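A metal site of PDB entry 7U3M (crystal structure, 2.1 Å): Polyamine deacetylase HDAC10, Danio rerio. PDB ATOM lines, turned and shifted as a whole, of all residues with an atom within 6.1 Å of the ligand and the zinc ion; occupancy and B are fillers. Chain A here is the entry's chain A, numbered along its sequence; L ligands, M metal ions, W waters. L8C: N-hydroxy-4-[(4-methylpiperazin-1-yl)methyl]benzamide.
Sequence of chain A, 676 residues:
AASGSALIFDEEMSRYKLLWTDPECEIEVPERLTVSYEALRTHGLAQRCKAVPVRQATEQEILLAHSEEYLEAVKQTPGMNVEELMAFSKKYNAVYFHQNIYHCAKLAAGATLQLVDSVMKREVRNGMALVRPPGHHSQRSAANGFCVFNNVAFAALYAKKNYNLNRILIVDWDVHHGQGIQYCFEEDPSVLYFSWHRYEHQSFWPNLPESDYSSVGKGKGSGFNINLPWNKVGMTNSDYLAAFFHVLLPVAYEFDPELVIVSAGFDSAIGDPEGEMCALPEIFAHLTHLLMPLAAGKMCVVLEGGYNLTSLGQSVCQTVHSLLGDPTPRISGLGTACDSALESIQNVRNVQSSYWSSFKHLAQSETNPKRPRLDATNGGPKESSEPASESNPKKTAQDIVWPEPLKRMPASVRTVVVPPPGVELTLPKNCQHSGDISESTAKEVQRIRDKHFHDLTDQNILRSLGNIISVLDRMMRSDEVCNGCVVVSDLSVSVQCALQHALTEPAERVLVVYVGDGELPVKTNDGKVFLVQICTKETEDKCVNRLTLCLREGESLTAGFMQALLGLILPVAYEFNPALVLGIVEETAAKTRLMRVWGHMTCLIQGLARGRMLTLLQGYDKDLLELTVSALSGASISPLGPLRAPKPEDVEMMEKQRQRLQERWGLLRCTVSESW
The side-chain hydroxyl (OH) of Tyr 307 sits at hydrogen-bond distance from a nitrogen (N15) of the ligand (2.4 Å). An oxygen (O14) of the ligand is in hydrogen-bond range of a ring nitrogen (NE2) of His 137 (3.1 Å). N05 of the ligand lies within salt-bridge range of OE2 of Glu 274, at 3.7 Å.
The side-chain carboxylate (OD1) of Asp 174 lies within hydrogen-bond range of the backbone NH (N) of Gly 305, 3.1 Å away. OD1 of Asp 267 is in hydrogen-bond range of N of Val 175, at 2.8 Å. The side-chain carboxylate (OE1) of Glu 274 lies within hydrogen-bond range of a ring nitrogen (NE2) of His 176 (3.0 Å). A ring nitrogen (NE2) of His 137 is in hydrogen-bond range of a ring nitrogen (NE2) of His 136, 3.3 Å away. N of His 137 is in hydrogen-bond range of SG of Cys 147 (3.5 Å). The backbone NH (N) of Phe 146 lies within hydrogen-bond range of the backbone carbonyl oxygen (O) of Ala 94 (2.9 Å). N of Gly 145 sits close to O of Ala 94 (3.3 Å). The side-chain sulfur of Cys 147 lies within hydrogen-bond range of the backbone carbonyl oxygen of Gly 145.
Residues that only touch the ligand: Phe 146 (3.3 Å), Gly 305 (3.4 Å), Trp 205 (3.4 Å), Gly 145 (3.6 Å), Glu 24 (3.6 Å), Phe 204 (3.9 Å), Ile 27 (3.96 Å) and Ala 94 (3.99 Å). Within 4 Å of the ligand: Glu 24, Ile 27, Ala 94, His 137, Gly 145, Phe 146, Asp 174, His 176, Phe 204, Trp 205, Asp 267, Glu 274, Gly 305 and Tyr 307. The nearest printed residue that does not touch the ligand is Gly 306 (4.4 Å).
Within 4 Å of the zinc ion: Asp 174, His 176 and Asp 267. The nearest printed residue that does not touch the zinc ion is His 136 (4.2 Å).
OD2 of Asp 174 is bound to the zinc ion. O16 of the ligand binds the zinc ion (2.0 Å). OD2 of Asp 267 is bound to the zinc ion, at 2.0 Å. The zinc ion is bound by water W1, at 2.1 Å. ND1 of His 176 binds the zinc ion, 2.2 Å away. The zinc ion has five donor atoms within binding distance. Slightly farther from the zinc ion lies the side-chain carboxylate (OD1) of Asp 174 (2.7 Å).
Water W1 lies within hydrogen-bond range of O14 of the ligand, NE2 of His 136, NE2 of His 137 and OD1 of Asp 174.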
ATOM      1  N   PRO A  23       9.019  10.370  13.686  1.00  0.00           N
ATOM      2  CA  PRO A  23       9.523  10.107  12.321  1.00  0.00           C
ATOM      3  C   PRO A  23      10.963  10.540  12.124  1.00  0.00           C
ATOM      4  O   PRO A  23      11.645   9.970  11.272  1.00  0.00           O
ATOM      5  CB  PRO A  23       8.554  10.912  11.428  1.00  0.00           C
ATOM      6  CG  PRO A  23       7.338  11.151  12.289  1.00  0.00           C
ATOM      7  CD  PRO A  23       7.869  11.283  13.690  1.00  0.00           C
ATOM      8  N   GLU A  24      11.448  11.513  12.901  1.00  0.00           N
ATOM      9  CA  GLU A  24      12.837  11.967  12.775  1.00  0.00           C
ATOM     10  C   GLU A  24      13.852  10.923  13.238  1.00  0.00           C
ATOM     11  O   GLU A  24      15.008  10.988  12.794  1.00  0.00           O
ATOM     12  CB  GLU A  24      13.036  13.261  13.558  1.00  0.00           C
ATOM     13  CG  GLU A  24      12.025  14.337  13.193  1.00  0.00           C
ATOM     14  CD  GLU A  24      12.304  14.940  11.824  1.00  0.00           C
ATOM     15  OE1 GLU A  24      13.035  15.955  11.752  1.00  0.00           O
ATOM     16  OE2 GLU A  24      11.795  14.389  10.822  1.00  0.00           O
ATOM     17  N   CYS A  25      13.468   9.984  14.112  1.00  0.00           N
ATOM     18  CA  CYS A  25      14.396   8.971  14.630  1.00  0.00           C
ATOM     19  C   CYS A  25      14.042   7.543  14.292  1.00  0.00           C
ATOM     20  O   CYS A  25      14.780   6.640  14.729  1.00  0.00           O
ATOM     21  CB  CYS A  25      14.534   9.057  16.167  1.00  0.00           C
ATOM     22  SG  CYS A  25      14.949  10.662  16.932  1.00  0.00           S
ATOM     23  N   ILE A  27      14.571   5.625  11.977  1.00  0.00           N
ATOM     24  CA  ILE A  27      15.528   4.830  11.201  1.00  0.00           C
ATOM     25  C   ILE A  27      16.683   4.257  12.007  1.00  0.00           C
ATOM     26  O   ILE A  27      17.430   3.407  11.481  1.00  0.00           O
ATOM     27  CB  ILE A  27      16.166   5.666  10.075  1.00  0.00           C
ATOM     28  CG1 ILE A  27      16.780   6.927  10.676  1.00  0.00           C
ATOM     29  CG2 ILE A  27      15.152   5.984   8.984  1.00  0.00           C
ATOM     30  CD1 ILE A  27      17.683   7.625   9.739  1.00  0.00           C
ATOM     31  N   ALA A  94      16.969  15.615  17.266  1.00  0.00           N
ATOM     32  CA  ALA A  94      16.969  14.315  16.572  1.00  0.00           C
ATOM     33  C   ALA A  94      17.719  13.230  17.360  1.00  0.00           C
ATOM     34  O   ALA A  94      18.665  12.608  16.877  1.00  0.00           O
ATOM     35  CB  ALA A  94      17.540  14.465  15.157  1.00  0.00           C
ATOM     36  N   PRO A 134      25.777   5.768  17.791  1.00  0.00           N
ATOM     37  CA  PRO A 134      26.892   6.443  17.115  1.00  0.00           C
ATOM     38  C   PRO A 134      27.377   7.650  17.892  1.00  0.00           C
ATOM     39  O   PRO A 134      26.804   7.980  18.941  1.00  0.00           O
ATOM     40  CB  PRO A 134      26.280   6.847  15.771  1.00  0.00           C
ATOM     41  CG  PRO A 134      24.817   7.110  16.126  1.00  0.00           C
ATOM     42  CD  PRO A 134      24.479   6.034  17.138  1.00  0.00           C
ATOM     43  N   HIS A 136      29.376  10.874  16.263  1.00  0.00           N
ATOM     44  CA  HIS A 136      30.091  12.049  15.759  1.00  0.00           C
ATOM     45  C   HIS A 136      29.285  13.350  15.822  1.00  0.00           C
ATOM     46  O   HIS A 136      29.891  14.421  15.768  1.00  0.00           O
ATOM     47  CB  HIS A 136      30.633  11.771  14.344  1.00  0.00           C
ATOM     48  CG  HIS A 136      29.582  11.608  13.284  1.00  0.00           C
ATOM     49  ND1 HIS A 136      29.830  11.899  11.950  1.00  0.00           N
ATOM     50  CD2 HIS A 136      28.302  11.161  13.331  1.00  0.00           C
ATOM     51  CE1 HIS A 136      28.742  11.644  11.237  1.00  0.00           C
ATOM     52  NE2 HIS A 136      27.799  11.208  12.056  1.00  0.00           N
ATOM     53  N   HIS A 137      27.967  13.298  16.010  1.00  0.00           N
ATOM     54  CA  HIS A 137      27.174  14.502  16.223  1.00  0.00           C
ATOM     55  C   HIS A 137      27.176  14.976  17.674  1.00  0.00           C
ATOM     56  O   HIS A 137      26.796  16.132  17.934  1.00  0.00           O
ATOM     57  CB  HIS A 137      25.729  14.278  15.784  1.00  0.00           C
ATOM     58  CG  HIS A 137      25.599  13.968  14.333  1.00  0.00           C
ATOM     59  ND1 HIS A 137      26.317  14.633  13.363  1.00  0.00           N
ATOM     60  CD2 HIS A 137      24.854  13.046  13.676  1.00  0.00           C
ATOM     61  CE1 HIS A 137      26.034  14.127  12.174  1.00  0.00           C
ATOM     62  NE2 HIS A 137      25.141  13.167  12.336  1.00  0.00           N
ATOM     63  N   GLY A 145      21.606  14.016  16.974  1.00  0.00           N
ATOM     64  CA  GLY A 145      21.561  13.095  15.858  1.00  0.00           C
ATOM     65  C   GLY A 145      21.900  11.651  16.236  1.00  0.00           C
ATOM     66  O   GLY A 145      22.877  11.111  15.726  1.00  0.00           O
ATOM     67  N   PHE A 146      21.126  11.061  17.151  1.00  0.00           N
ATOM     68  CA  PHE A 146      21.280   9.673  17.619  1.00  0.00           C
ATOM     69  C   PHE A 146      22.502   9.445  18.497  1.00  0.00           C
ATOM     70  O   PHE A 146      22.635   8.369  19.072  1.00  0.00           O
ATOM     71  CB  PHE A 146      21.322   8.691  16.443  1.00  0.00           C
ATOM     72  CG  PHE A 146      20.166   8.815  15.519  1.00  0.00           C
ATOM     73  CD1 PHE A 146      18.914   9.122  16.014  1.00  0.00           C
ATOM     74  CD2 PHE A 146      20.321   8.646  14.159  1.00  0.00           C
ATOM     75  CE1 PHE A 146      17.836   9.259  15.161  1.00  0.00           C
ATOM     76  CE2 PHE A 146      19.247   8.766  13.304  1.00  0.00           C
ATOM     77  CZ  PHE A 146      18.000   9.086  13.803  1.00  0.00           C
ATOM     78  N   CYS A 147      23.375  10.450  18.623  1.00  0.00           N
ATOM     79  CA  CYS A 147      24.623  10.317  19.362  1.00  0.00           C
ATOM     80  C   CYS A 147      24.485  10.843  20.789  1.00  0.00           C
ATOM     81  O   CYS A 147      23.894  11.905  21.020  1.00  0.00           O
ATOM     82  CB  CYS A 147      25.751  11.087  18.663  1.00  0.00           C
ATOM     83  SG  CYS A 147      25.913  10.646  16.930  1.00  0.00           S
ATOM     84  N   ASP A 174      30.917   9.152   6.894  1.00  0.00           N
ATOM     85  CA  ASP A 174      29.469   9.235   7.076  1.00  0.00           C
ATOM     86  C   ASP A 174      28.903  10.322   6.163  1.00  0.00           C
ATOM     87  O   ASP A 174      29.580  11.297   5.850  1.00  0.00           O
ATOM     88  CB  ASP A 174      29.166   9.575   8.538  1.00  0.00           C
ATOM     89  CG  ASP A 174      27.720   9.386   8.893  1.00  0.00           C
ATOM     90  OD1 ASP A 174      27.396   8.329   9.463  1.00  0.00           O
ATOM     91  OD2 ASP A 174      26.908  10.309   8.634  1.00  0.00           O
ATOM     92  N   VAL A 175      27.643  10.150   5.745  1.00  0.00           N
ATOM     93  CA  VAL A 175      27.023  11.124   4.854  1.00  0.00           C
ATOM     94  C   VAL A 175      26.634  12.425   5.552  1.00  0.00           C
ATOM     95  O   VAL A 175      26.309  13.396   4.884  1.00  0.00           O
ATOM     96  CB  VAL A 175      25.787  10.530   4.150  1.00  0.00           C
ATOM     97  CG1 VAL A 175      24.527  10.681   5.040  1.00  0.00           C
ATOM     98  CG2 VAL A 175      25.587  11.212   2.788  1.00  0.00           C
ATOM     99  N   HIS A 176      26.647  12.455   6.883  1.00  0.00           N
ATOM    100  CA  HIS A 176      26.328  13.631   7.676  1.00  0.00           C
ATOM    101  C   HIS A 176      27.606  14.277   8.185  1.00  0.00           C
ATOM    102  O   HIS A 176      28.643  13.611   8.329  1.00  0.00           O
ATOM    103  CB  HIS A 176      25.425  13.265   8.859  1.00  0.00           C
ATOM    104  CG  HIS A 176      24.088  12.717   8.457  1.00  0.00           C
ATOM    105  ND1 HIS A 176      23.836  11.376   8.331  1.00  0.00           N
ATOM    106  CD2 HIS A 176      22.929  13.347   8.141  1.00  0.00           C
ATOM    107  CE1 HIS A 176      22.578  11.186   7.970  1.00  0.00           C
ATOM    108  NE2 HIS A 176      22.005  12.367   7.839  1.00  0.00           N
ATOM    109  N   PHE A 204      20.341  20.876   4.220  1.00  0.00           N
ATOM    110  CA  PHE A 204      20.280  19.523   4.781  1.00  0.00           C
ATOM    111  C   PHE A 204      20.794  19.503   6.215  1.00  0.00           C
ATOM    112  O   PHE A 204      21.797  20.141   6.542  1.00  0.00           O
ATOM    113  CB  PHE A 204      21.064  18.522   3.936  1.00  0.00           C
ATOM    114  CG  PHE A 204      20.725  17.095   4.249  1.00  0.00           C
ATOM    115  CD1 PHE A 204      19.488  16.574   3.897  1.00  0.00           C
ATOM    116  CD2 PHE A 204      21.640  16.279   4.906  1.00  0.00           C
ATOM    117  CE1 PHE A 204      19.167  15.236   4.202  1.00  0.00           C
ATOM    118  CE2 PHE A 204      21.337  14.953   5.204  1.00  0.00           C
ATOM    119  CZ  PHE A 204      20.091  14.435   4.850  1.00  0.00           C
ATOM    120  N   TRP A 205      20.088  18.758   7.068  1.00  0.00           N
ATOM    121  CA  TRP A 205      20.461  18.574   8.465  1.00  0.00           C
ATOM    122  C   TRP A 205      21.954  18.234   8.585  1.00  0.00           C
ATOM    123  O   TRP A 205      22.468  17.413   7.807  1.00  0.00           O
ATOM    124  CB  TRP A 205      19.583  17.459   9.067  1.00  0.00           C
ATOM    125  CG  TRP A 205      19.656  17.391  10.548  1.00  0.00           C
ATOM    126  CD1 TRP A 205      18.778  17.942  11.442  1.00  0.00           C
ATOM    127  CD2 TRP A 205      20.665  16.743  11.311  1.00  0.00           C
ATOM    128  NE1 TRP A 205      19.186  17.678  12.722  1.00  0.00           N
ATOM    129  CE2 TRP A 205      20.350  16.954  12.676  1.00  0.00           C
ATOM    130  CE3 TRP A 205      21.818  16.007  10.981  1.00  0.00           C
ATOM    131  CZ2 TRP A 205      21.133  16.431  13.711  1.00  0.00           C
ATOM    132  CZ3 TRP A 205      22.607  15.503  12.028  1.00  0.00           C
ATOM    133  CH2 TRP A 205      22.254  15.718  13.368  1.00  0.00           C
ATOM    134  N   GLY A 265      30.454   5.914   8.786  1.00  0.00           N
ATOM    135  CA  GLY A 265      29.039   5.803   8.535  1.00  0.00           C
ATOM    136  C   GLY A 265      28.868   5.354   7.098  1.00  0.00           C
ATOM    137  O   GLY A 265      29.512   5.874   6.183  1.00  0.00           O
ATOM    138  N   ASP A 267      25.839   5.391   5.671  1.00  0.00           N
ATOM    139  CA  ASP A 267      24.744   6.106   5.023  1.00  0.00           C
ATOM    140  C   ASP A 267      25.218   6.908   3.819  1.00  0.00           C
ATOM    141  O   ASP A 267      24.376   7.495   3.132  1.00  0.00           O
ATOM    142  CB  ASP A 267      24.019   7.009   6.016  1.00  0.00           C
ATOM    143  CG  ASP A 267      24.950   7.828   6.890  1.00  0.00           C
ATOM    144  OD1 ASP A 267      26.161   7.938   6.591  1.00  0.00           O
ATOM    145  OD2 ASP A 267      24.470   8.379   7.896  1.00  0.00           O
ATOM    146  N   GLU A 274      18.782   8.113   4.044  1.00  0.00           N
ATOM    147  CA  GLU A 274      19.212   9.425   4.517  1.00  0.00           C
ATOM    148  C   GLU A 274      20.168  10.098   3.545  1.00  0.00           C
ATOM    149  O   GLU A 274      20.053  11.308   3.309  1.00  0.00           O
ATOM    150  CB  GLU A 274      19.889   9.316   5.892  1.00  0.00           C
ATOM    151  CG  GLU A 274      18.929   9.409   7.026  1.00  0.00           C
ATOM    152  CD  GLU A 274      18.382  10.812   7.217  1.00  0.00           C
ATOM    153  OE1 GLU A 274      19.148  11.796   7.127  1.00  0.00           O
ATOM    154  OE2 GLU A 274      17.170  10.925   7.453  1.00  0.00           O
ATOM    155  N   GLU A 304      29.472   4.594  12.538  1.00  0.00           N
ATOM    156  CA  GLU A 304      28.562   5.683  12.859  1.00  0.00           C
ATOM    157  C   GLU A 304      27.190   5.302  12.336  1.00  0.00           C
ATOM    158  O   GLU A 304      26.446   4.562  13.013  1.00  0.00           O
ATOM    159  CB  GLU A 304      29.093   7.015  12.292  1.00  0.00           C
ATOM    160  CG  GLU A 304      30.479   7.415  12.838  1.00  0.00           C
ATOM    161  CD  GLU A 304      30.403   8.087  14.222  1.00  0.00           C
ATOM    162  OE1 GLU A 304      29.311   8.167  14.811  1.00  0.00           O
ATOM    163  OE2 GLU A 304      31.453   8.555  14.718  1.00  0.00           O
ATOM    164  N   GLY A 305      26.785   5.749  11.145  1.00  0.00           N
ATOM    165  CA  GLY A 305      25.458   5.529  10.629  1.00  0.00           C
ATOM    166  C   GLY A 305      25.417   4.508   9.503  1.00  0.00           C
ATOM    167  O   GLY A 305      26.358   3.761   9.257  1.00  0.00           O
ATOM    168  N   GLY A 306      24.273   4.494   8.811  1.00  0.00           N
ATOM    169  CA  GLY A 306      24.006   3.526   7.756  1.00  0.00           C
ATOM    170  C   GLY A 306      22.708   2.805   8.060  1.00  0.00           C
ATOM    171  O   GLY A 306      22.625   2.076   9.042  1.00  0.00           O
ATOM    172  N   TYR A 307      21.676   3.045   7.249  1.00  0.00           N
ATOM    173  CA  TYR A 307      20.323   2.663   7.610  1.00  0.00           C
ATOM    174  C   TYR A 307      19.625   1.736   6.628  1.00  0.00           C
ATOM    175  O   TYR A 307      18.534   1.266   6.938  1.00  0.00           O
ATOM    176  CB  TYR A 307      19.472   3.926   7.802  1.00  0.00           C
ATOM    177  CG  TYR A 307      20.169   4.837   8.758  1.00  0.00           C
ATOM    178  CD1 TYR A 307      20.106   4.579  10.123  1.00  0.00           C
ATOM    179  CD2 TYR A 307      20.953   5.886   8.303  1.00  0.00           C
ATOM    180  CE1 TYR A 307      20.773   5.364  11.016  1.00  0.00           C
ATOM    181  CE2 TYR A 307      21.620   6.700   9.201  1.00  0.00           C
ATOM    182  CZ  TYR A 307      21.526   6.436  10.548  1.00  0.00           C
ATOM    183  OH  TYR A 307      22.184   7.230  11.448  1.00  0.00           O
HETATM  184  C10 L8C L   1      21.179  11.162  11.412  1.00  0.00           C
HETATM  185  C13 L8C L   1      22.514  10.404  11.426  1.00  0.00           C
HETATM  186  C17 L8C L   1      15.748  13.855   9.959  1.00  0.00           C
HETATM  187  C01 L8C L   1      16.090  14.335   6.416  1.00  0.00           C
HETATM  188  C03 L8C L   1      17.603  14.576   8.005  1.00  0.00           C
HETATM  189  C04 L8C L   1      17.934  14.300   9.470  1.00  0.00           C
HETATM  190  C06 L8C L   1      17.377  13.259  11.354  1.00  0.00           C
HETATM  191  C07 L8C L   1      18.740  12.529  11.396  1.00  0.00           C
HETATM  192  C08 L8C L   1      18.881  11.266  10.743  1.00  0.00           C
HETATM  193  C09 L8C L   1      20.114  10.601  10.751  1.00  0.00           C
HETATM  194  C11 L8C L   1      21.057  12.432  12.095  1.00  0.00           C
HETATM  195  C12 L8C L   1      19.841  13.098  12.062  1.00  0.00           C
HETATM  196  C18 L8C L   1      15.342  14.110   8.498  1.00  0.00           C
HETATM  197  N02 L8C L   1      16.276  14.653   7.674  1.00  0.00           N
HETATM  198  N05 L8C L   1      17.049  13.464  10.094  1.00  0.00           N
HETATM  199  N15 L8C L   1      22.763   9.357  10.396  1.00  0.00           N
HETATM  200  O14 L8C L   1      23.327  10.645  12.204  1.00  0.00           O
HETATM  201  O16 L8C L   1      24.017   8.638  10.401  1.00  0.00           O
HETATM  202 ZN    ZN M   1      25.110   9.824   9.201  1.00  0.00          ZN
HETATM  203  O   HOH W   1      25.565  10.613  11.135  1.00  0.00           O
HETATM  204  O   HOH W   2      15.345  17.224   9.560  1.00  0.00           O
